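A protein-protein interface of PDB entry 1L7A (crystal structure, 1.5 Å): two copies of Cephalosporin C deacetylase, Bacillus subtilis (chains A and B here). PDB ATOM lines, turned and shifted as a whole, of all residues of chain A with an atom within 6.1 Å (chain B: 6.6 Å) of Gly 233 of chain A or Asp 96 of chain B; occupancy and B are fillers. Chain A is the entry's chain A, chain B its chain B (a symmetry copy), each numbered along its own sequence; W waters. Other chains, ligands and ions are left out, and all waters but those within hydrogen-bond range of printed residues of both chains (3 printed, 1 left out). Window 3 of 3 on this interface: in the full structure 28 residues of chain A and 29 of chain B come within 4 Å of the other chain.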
ATOM      1  N   PHE A 228     -29.453  -7.648 -20.175  1.00  0.00           N
ATOM      2  CA  PHE A 228     -29.021  -6.675 -19.189  1.00  0.00           C
ATOM      3  C   PHE A 228     -28.068  -7.318 -18.204  1.00  0.00           C
ATOM      4  O   PHE A 228     -27.071  -6.676 -17.846  1.00  0.00           O
ATOM      5  CB  PHE A 228     -30.249  -6.113 -18.499  1.00  0.00           C
ATOM      6  CG  PHE A 228     -29.962  -5.163 -17.366  1.00  0.00           C
ATOM      7  CD1 PHE A 228     -29.560  -3.858 -17.631  1.00  0.00           C
ATOM      8  CD2 PHE A 228     -30.098  -5.574 -16.061  1.00  0.00           C
ATOM      9  CE1 PHE A 228     -29.330  -2.988 -16.575  1.00  0.00           C
ATOM     10  CE2 PHE A 228     -29.874  -4.702 -15.010  1.00  0.00           C
ATOM     11  CZ  PHE A 228     -29.474  -3.408 -15.272  1.00  0.00           C
ATOM     12  N   PHE A 229     -28.289  -8.558 -17.782  1.00  0.00           N
ATOM     13  CA  PHE A 229     -27.384  -9.217 -16.836  1.00  0.00           C
ATOM     14  C   PHE A 229     -26.062  -9.503 -17.522  1.00  0.00           C
ATOM     15  O   PHE A 229     -25.049  -9.560 -16.827  1.00  0.00           O
ATOM     16  CB  PHE A 229     -27.995 -10.472 -16.209  1.00  0.00           C
ATOM     17  CG  PHE A 229     -29.235 -10.209 -15.405  1.00  0.00           C
ATOM     18  CD1 PHE A 229     -29.391  -9.038 -14.695  1.00  0.00           C
ATOM     19  CD2 PHE A 229     -30.265 -11.144 -15.358  1.00  0.00           C
ATOM     20  CE1 PHE A 229     -30.534  -8.785 -13.959  1.00  0.00           C
ATOM     21  CE2 PHE A 229     -31.409 -10.907 -14.622  1.00  0.00           C
ATOM     22  CZ  PHE A 229     -31.544  -9.724 -13.919  1.00  0.00           C
ATOM     23  N   ARG A 230     -26.032  -9.729 -18.832  1.00  0.00           N
ATOM     24  CA  ARG A 230     -24.773  -9.938 -19.530  1.00  0.00           C
ATOM     25  C   ARG A 230     -23.953  -8.647 -19.499  1.00  0.00           C
ATOM     26  O   ARG A 230     -22.728  -8.704 -19.409  1.00  0.00           O
ATOM     27  CB  ARG A 230     -25.016 -10.359 -20.991  1.00  0.00           C
ATOM     28  CG  ARG A 230     -25.604 -11.768 -21.103  1.00  0.00           C
ATOM     29  CD  ARG A 230     -26.111 -12.053 -22.507  1.00  0.00           C
ATOM     30  NE  ARG A 230     -25.162 -11.844 -23.580  1.00  0.00           N
ATOM     31  CZ  ARG A 230     -24.181 -12.670 -23.928  1.00  0.00           C
ATOM     32  NH1 ARG A 230     -23.973 -13.822 -23.279  1.00  0.00           N
ATOM     33  NH2 ARG A 230     -23.407 -12.291 -24.949  1.00  0.00           N
ATOM     34  N   ARG A 231     -24.639  -7.506 -19.610  1.00  0.00           N
ATOM     35  CA  ARG A 231     -23.930  -6.228 -19.663  1.00  0.00           C
ATOM     36  C   ARG A 231     -23.672  -5.566 -18.323  1.00  0.00           C
ATOM     37  O   ARG A 231     -22.890  -4.624 -18.248  1.00  0.00           O
ATOM     38  CB  ARG A 231     -24.767  -5.294 -20.551  1.00  0.00           C
ATOM     39  CG  ARG A 231     -24.774  -5.633 -22.031  1.00  0.00           C
ATOM     40  CD  ARG A 231     -25.998  -5.084 -22.765  1.00  0.00           C
ATOM     41  NE  ARG A 231     -25.824  -5.339 -24.187  1.00  0.00           N
ATOM     42  CZ  ARG A 231     -25.955  -6.509 -24.785  1.00  0.00           C
ATOM     43  NH1 ARG A 231     -26.299  -7.577 -24.064  1.00  0.00           N
ATOM     44  NH2 ARG A 231     -25.749  -6.626 -26.081  1.00  0.00           N
ATOM     45  N   ASN A 232     -24.284  -6.089 -17.272  1.00  0.00           N
ATOM     46  CA  ASN A 232     -24.181  -5.552 -15.921  1.00  0.00           C
ATOM     47  C   ASN A 232     -24.130  -6.815 -15.068  1.00  0.00           C
ATOM     48  O   ASN A 232     -25.165  -7.234 -14.561  1.00  0.00           O
ATOM     49  CB  ASN A 232     -25.421  -4.725 -15.599  1.00  0.00           C
ATOM     50  CG  ASN A 232     -25.663  -3.640 -16.625  1.00  0.00           C
ATOM     51  OD1 ASN A 232     -26.245  -3.803 -17.698  1.00  0.00           O
ATOM     52  ND2 ASN A 232     -25.184  -2.453 -16.300  1.00  0.00           N
ATOM     53  N   GLY A 233     -22.953  -7.407 -14.936  1.00  0.00           N
ATOM     54  CA  GLY A 233     -22.797  -8.683 -14.269  1.00  0.00           C
ATOM     55  C   GLY A 233     -22.681  -8.840 -12.774  1.00  0.00           C
ATOM     56  O   GLY A 233     -22.571  -9.986 -12.344  1.00  0.00           O
ATOM     57  N   SER A 234     -22.731  -7.741 -12.044  1.00  0.00           N
ATOM     58  CA  SER A 234     -22.641  -7.847 -10.588  1.00  0.00           C
ATOM     59  C   SER A 234     -23.759  -8.696 -10.034  1.00  0.00           C
ATOM     60  O   SER A 234     -24.921  -8.518 -10.399  1.00  0.00           O
ATOM     61  CB  SER A 234     -22.868  -6.421 -10.081  1.00  0.00           C
ATOM     62  OG  SER A 234     -23.296  -6.423  -8.736  1.00  0.00           O
ATOM     63  N   PRO A 235     -23.454  -9.634  -9.145  1.00  0.00           N
ATOM     64  CA  PRO A 235     -24.475 -10.463  -8.525  1.00  0.00           C
ATOM     65  C   PRO A 235     -25.566  -9.653  -7.863  1.00  0.00           C
ATOM     66  O   PRO A 235     -26.753  -9.992  -7.928  1.00  0.00           O
ATOM     67  CB  PRO A 235     -23.623 -11.323  -7.590  1.00  0.00           C
ATOM     68  CG  PRO A 235     -22.310 -11.386  -8.289  1.00  0.00           C
ATOM     69  CD  PRO A 235     -22.069  -9.960  -8.718  1.00  0.00           C
ATOM     70  N   GLU A 236     -25.245  -8.551  -7.197  1.00  0.00           N
ATOM     71  CA  GLU A 236     -26.189  -7.696  -6.503  1.00  0.00           C
ATOM     72  C   GLU A 236     -27.134  -7.073  -7.522  1.00  0.00           C
ATOM     73  O   GLU A 236     -28.303  -6.856  -7.200  1.00  0.00           O
ATOM     74  CB  GLU A 236     -25.482  -6.629  -5.670  1.00  0.00           C
ATOM     75  CG  GLU A 236     -24.533  -7.133  -4.604  1.00  0.00           C
ATOM     76  CD  GLU A 236     -23.092  -7.390  -5.000  1.00  0.00           C
ATOM     77  OE1 GLU A 236     -22.670  -7.366  -6.175  1.00  0.00           O
ATOM     78  OE2 GLU A 236     -22.311  -7.635  -4.050  1.00  0.00           O
ATOM     79  N   THR A 237     -26.625  -6.742  -8.704  1.00  0.00           N
ATOM     80  CA  THR A 237     -27.469  -6.143  -9.730  1.00  0.00           C
ATOM     81  C   THR A 237     -28.605  -7.069 -10.138  1.00  0.00           C
ATOM     82  O   THR A 237     -29.764  -6.667 -10.312  1.00  0.00           O
ATOM     83  CB  THR A 237     -26.634  -5.772 -10.962  1.00  0.00           C
ATOM     84  OG1 THR A 237     -25.779  -4.699 -10.529  1.00  0.00           O
ATOM     85  CG2 THR A 237     -27.529  -5.387 -12.125  1.00  0.00           C
ATOM     86  N   TRP B  72     -14.900   4.033 -16.873  1.00  0.00           N
ATOM     87  CA  TRP B  72     -13.666   3.671 -16.196  1.00  0.00           C
ATOM     88  C   TRP B  72     -12.571   4.583 -16.721  1.00  0.00           C
ATOM     89  O   TRP B  72     -12.503   4.909 -17.912  1.00  0.00           O
ATOM     90  CB  TRP B  72     -13.274   2.224 -16.415  1.00  0.00           C
ATOM     91  CG  TRP B  72     -14.376   1.279 -16.032  1.00  0.00           C
ATOM     92  CD1 TRP B  72     -15.043   0.454 -16.882  1.00  0.00           C
ATOM     93  CD2 TRP B  72     -14.908   1.051 -14.728  1.00  0.00           C
ATOM     94  NE1 TRP B  72     -15.984  -0.260 -16.184  1.00  0.00           N
ATOM     95  CE2 TRP B  72     -15.924   0.086 -14.862  1.00  0.00           C
ATOM     96  CE3 TRP B  72     -14.654   1.586 -13.466  1.00  0.00           C
ATOM     97  CZ2 TRP B  72     -16.662  -0.381 -13.775  1.00  0.00           C
ATOM     98  CZ3 TRP B  72     -15.391   1.127 -12.387  1.00  0.00           C
ATOM     99  CH2 TRP B  72     -16.380   0.145 -12.548  1.00  0.00           C
ATOM    100  N   SER B  94     -21.483  -2.378 -24.667  1.00  0.00           N
ATOM    101  CA  SER B  94     -20.578  -2.284 -23.546  1.00  0.00           C
ATOM    102  C   SER B  94     -21.050  -3.324 -22.526  1.00  0.00           C
ATOM    103  O   SER B  94     -22.222  -3.463 -22.138  1.00  0.00           O
ATOM    104  CB  SER B  94     -20.631  -0.900 -22.916  1.00  0.00           C
ATOM    105  OG  SER B  94     -19.729  -0.910 -21.820  1.00  0.00           O
ATOM    106  N   TYR B  95     -20.089  -4.132 -22.109  1.00  0.00           N
ATOM    107  CA  TYR B  95     -20.294  -5.178 -21.104  1.00  0.00           C
ATOM    108  C   TYR B  95     -19.467  -4.720 -19.903  1.00  0.00           C
ATOM    109  O   TYR B  95     -18.240  -4.836 -19.869  1.00  0.00           O
ATOM    110  CB  TYR B  95     -19.852  -6.556 -21.589  1.00  0.00           C
ATOM    111  CG  TYR B  95     -20.752  -7.191 -22.620  1.00  0.00           C
ATOM    112  CD1 TYR B  95     -20.936  -6.715 -23.904  1.00  0.00           C
ATOM    113  CD2 TYR B  95     -21.401  -8.365 -22.229  1.00  0.00           C
ATOM    114  CE1 TYR B  95     -21.787  -7.384 -24.779  1.00  0.00           C
ATOM    115  CE2 TYR B  95     -22.233  -9.041 -23.108  1.00  0.00           C
ATOM    116  CZ  TYR B  95     -22.420  -8.529 -24.365  1.00  0.00           C
ATOM    117  OH  TYR B  95     -23.257  -9.243 -25.210  1.00  0.00           O
ATOM    118  N   ASP B  96     -20.172  -4.162 -18.938  1.00  0.00           N
ATOM    119  CA  ASP B  96     -19.554  -3.628 -17.726  1.00  0.00           C
ATOM    120  C   ASP B  96     -18.474  -2.577 -18.013  1.00  0.00           C
ATOM    121  O   ASP B  96     -17.545  -2.408 -17.228  1.00  0.00           O
ATOM    122  CB  ASP B  96     -19.107  -4.753 -16.788  1.00  0.00           C
ATOM    123  CG  ASP B  96     -20.290  -5.279 -15.979  1.00  0.00           C
ATOM    124  OD1 ASP B  96     -20.510  -6.520 -16.004  1.00  0.00           O
ATOM    125  OD2 ASP B  96     -20.957  -4.471 -15.292  1.00  0.00           O
ATOM    126  N   GLY B  97     -18.601  -1.859 -19.112  1.00  0.00           N
ATOM    127  CA  GLY B  97     -17.689  -0.771 -19.441  1.00  0.00           C
ATOM    128  C   GLY B  97     -16.319  -1.085 -19.976  1.00  0.00           C
ATOM    129  O   GLY B  97     -15.498  -0.162 -20.075  1.00  0.00           O
ATOM    130  N   GLU B  98     -16.000  -2.321 -20.318  1.00  0.00           N
ATOM    131  CA  GLU B  98     -14.726  -2.702 -20.890  1.00  0.00           C
ATOM    132  C   GLU B  98     -13.548  -2.257 -20.028  1.00  0.00           C
ATOM    133  O   GLU B  98     -12.535  -1.731 -20.516  1.00  0.00           O
ATOM    134  CB  GLU B  98     -14.564  -2.059 -22.274  1.00  0.00           C
ATOM    135  CG  GLU B  98     -15.483  -2.648 -23.328  1.00  0.00           C
ATOM    136  CD  GLU B  98     -16.952  -2.504 -23.044  1.00  0.00           C
ATOM    137  OE1 GLU B  98     -17.372  -1.339 -22.924  1.00  0.00           O
ATOM    138  OE2 GLU B  98     -17.572  -3.584 -22.956  1.00  0.00           O
ATOM    139  N   ILE B  99     -13.680  -2.564 -18.748  1.00  0.00           N
ATOM    140  CA  ILE B  99     -12.625  -2.138 -17.805  1.00  0.00           C
ATOM    141  C   ILE B  99     -11.269  -2.686 -18.187  1.00  0.00           C
ATOM    142  O   ILE B  99     -10.266  -1.975 -18.079  1.00  0.00           O
ATOM    143  CB  ILE B  99     -13.026  -2.448 -16.359  1.00  0.00           C
ATOM    144  CG1 ILE B  99     -12.101  -1.716 -15.383  1.00  0.00           C
ATOM    145  CG2 ILE B  99     -13.043  -3.941 -16.034  1.00  0.00           C
ATOM    146  CD1 ILE B  99     -12.561  -1.755 -13.932  1.00  0.00           C
ATOM    147  N   LEU B 116     -19.036   5.886 -21.065  1.00  0.00           N
ATOM    148  CA  LEU B 116     -20.166   4.949 -21.276  1.00  0.00           C
ATOM    149  C   LEU B 116     -21.350   5.786 -21.728  1.00  0.00           C
ATOM    150  O   LEU B 116     -21.670   6.842 -21.153  1.00  0.00           O
ATOM    151  CB  LEU B 116     -20.352   4.139 -19.999  1.00  0.00           C
ATOM    152  CG  LEU B 116     -19.072   3.430 -19.564  1.00  0.00           C
ATOM    153  CD1 LEU B 116     -19.300   2.688 -18.249  1.00  0.00           C
ATOM    154  CD2 LEU B 116     -18.555   2.490 -20.636  1.00  0.00           C
ATOM    155  N   GLN B 121     -25.249   2.111 -20.889  1.00  0.00           N
ATOM    156  CA  GLN B 121     -24.514   1.469 -19.801  1.00  0.00           C
ATOM    157  C   GLN B 121     -24.061   2.464 -18.722  1.00  0.00           C
ATOM    158  O   GLN B 121     -23.309   3.398 -18.969  1.00  0.00           O
ATOM    159  CB  GLN B 121     -23.295   0.768 -20.408  1.00  0.00           C
ATOM    160  CG  GLN B 121     -22.224   0.444 -19.365  1.00  0.00           C
ATOM    161  CD  GLN B 121     -22.426  -0.968 -18.868  1.00  0.00           C
ATOM    162  OE1 GLN B 121     -23.163  -1.769 -19.419  1.00  0.00           O
ATOM    163  NE2 GLN B 121     -21.725  -1.255 -17.753  1.00  0.00           N
ATOM    164  N   ARG B 122     -24.584   2.258 -17.495  1.00  0.00           N
ATOM    165  CA  ARG B 122     -24.124   3.039 -16.345  1.00  0.00           C
ATOM    166  C   ARG B 122     -24.431   4.537 -16.467  1.00  0.00           C
ATOM    167  O   ARG B 122     -24.995   5.156 -15.574  1.00  0.00           O
ATOM    168  CB  ARG B 122     -22.619   2.821 -16.183  1.00  0.00           C
ATOM    169  CG  ARG B 122     -22.308   1.663 -15.234  1.00  0.00           C
ATOM    170  CD  ARG B 122     -20.884   1.122 -15.416  1.00  0.00           C
ATOM    171  NE  ARG B 122     -20.529   0.243 -14.299  1.00  0.00           N
ATOM    172  CZ  ARG B 122     -20.890  -1.052 -14.391  1.00  0.00           C
ATOM    173  NH1 ARG B 122     -21.508  -1.494 -15.472  1.00  0.00           N
ATOM    174  NH2 ARG B 122     -20.659  -1.877 -13.366  1.00  0.00           N
HETATM  175  O   HOH W   1     -25.949   0.028 -17.188  1.00  0.00           O
HETATM  176  O   HOH W   2     -24.558  -1.497 -13.884  1.00  0.00           O
HETATM  177  O   HOH W   3     -20.352  -8.250 -18.233  1.00  0.00           O
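The guanidinium group of Arg 230 of chain A lies within hydrogen-bond range of the side-chain hydroxyl of Tyr 95 of chain B (3.1 Å). The side-chain carboxylate (OD1) of Asp 96 of chain B lies within hydrogen-bond range of the backbone NH (N) of Gly 233 of chain A, 2.8 Å away. N of Asp 96 of chain B lies within hydrogen-bond range of O of Arg 231 of chain A. The side-chain amide oxygen (OE1) of Gln 121 of chain B lies close to the backbone carbonyl oxygen (O) of Arg 231 of chain A, 3.1 Å away.
The backbone carbonyl oxygen (O) of Ser 94 of chain B sits close to the side-chain amide oxygen (OE1) of Gln 121 of chain B, 3.3 Å away. OE2 of Glu 98 of chain B sits at hydrogen-bond distance from N of Tyr 95 of chain B (2.7 Å). The side-chain amide oxygen (OD1) of Asn 232 of chain A lies close to the backbone carbonyl oxygen (O) of Phe 228 of chain A, at 3.0 Å. The side-chain carboxylate (OE1) of Glu 98 of chain B sits at hydrogen-bond distance from the side-chain hydroxyl (OG) of Ser 94 of chain B, 2.6 Å away. The side-chain hydroxyl of Ser 94 of chain B lies within hydrogen-bond range of the backbone NH of Gly 97 of chain B (3.1 Å). The side-chain amide nitrogen of Gln 121 of chain B sits close to the backbone NH of Gly 97 of chain B (3.5 Å).
Arg 231 of chain A touches Ser 94 of chain B. Arg 231 of chain A touches Tyr 95 of chain B. Asp 96 of chain B touches Asn 232 of chain A. Asn 232 of chain A touches Gln 121 of chain B. Asn 232 of chain A touches Arg 122 of chain B.
Of chain B, only Asp 96 (2.8 Å) comes within 4 Å of Gly 233 of chain A. Of chain A, only Arg 231, Asn 232 and Gly 233 come within 4 Å of Asp 96 of chain B. Of the printed residues of chain A, Tyr 95 of chain B touches Arg 230 and Arg 231. Printed residues of chain B within 4 Å of Arg 231 of chain A: Ser 94, Tyr 95, Asp 96 and Gln 121. Of the printed residues of chain A, Ser 94 of chain B touches Arg 231. The nearest residue of chain A that does not touch Asp 96 of chain B is Arg 230 of chain A (4.6 Å). The nearest printed residue of chain B that does not touch Arg 231 of chain A is Arg 122 of chain B (4.4 Å).
Of the 10 printed residues of chain B, 5 touch a printed residue of chain A. Hydrophobic or aromatic side chains of chain B that line the printed part of chain A: Tyr 95. Printed residues of chain A that touch a printed residue of chain B: Arg 230, Arg 231, Asn 232 and Gly 233. Along chain A the printed residues that touch a printed residue of chain B span positions 230 to 233.
No position is printed for both chains. Of the 9 pairs that touch across the chains among the printed residues, none has its exchanged pair printed and touching as well.
Water W1 bridges the backbone NH of Arg 122 of chain B (2.6 Å) and the side-chain amide nitrogen of Asn 232 of chain A (2.7 Å). Water W2 bridges ND2 of Asn 232 of chain A (2.7 Å) and NH1 of Arg 122 of chain B (3.4 Å). Water W3 lies within hydrogen-bond range of the backbone carbonyl oxygen of Arg 230 of chain A (2.7 Å) and the side-chain carboxylate of Asp 96 of chain B (2.8 Å).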
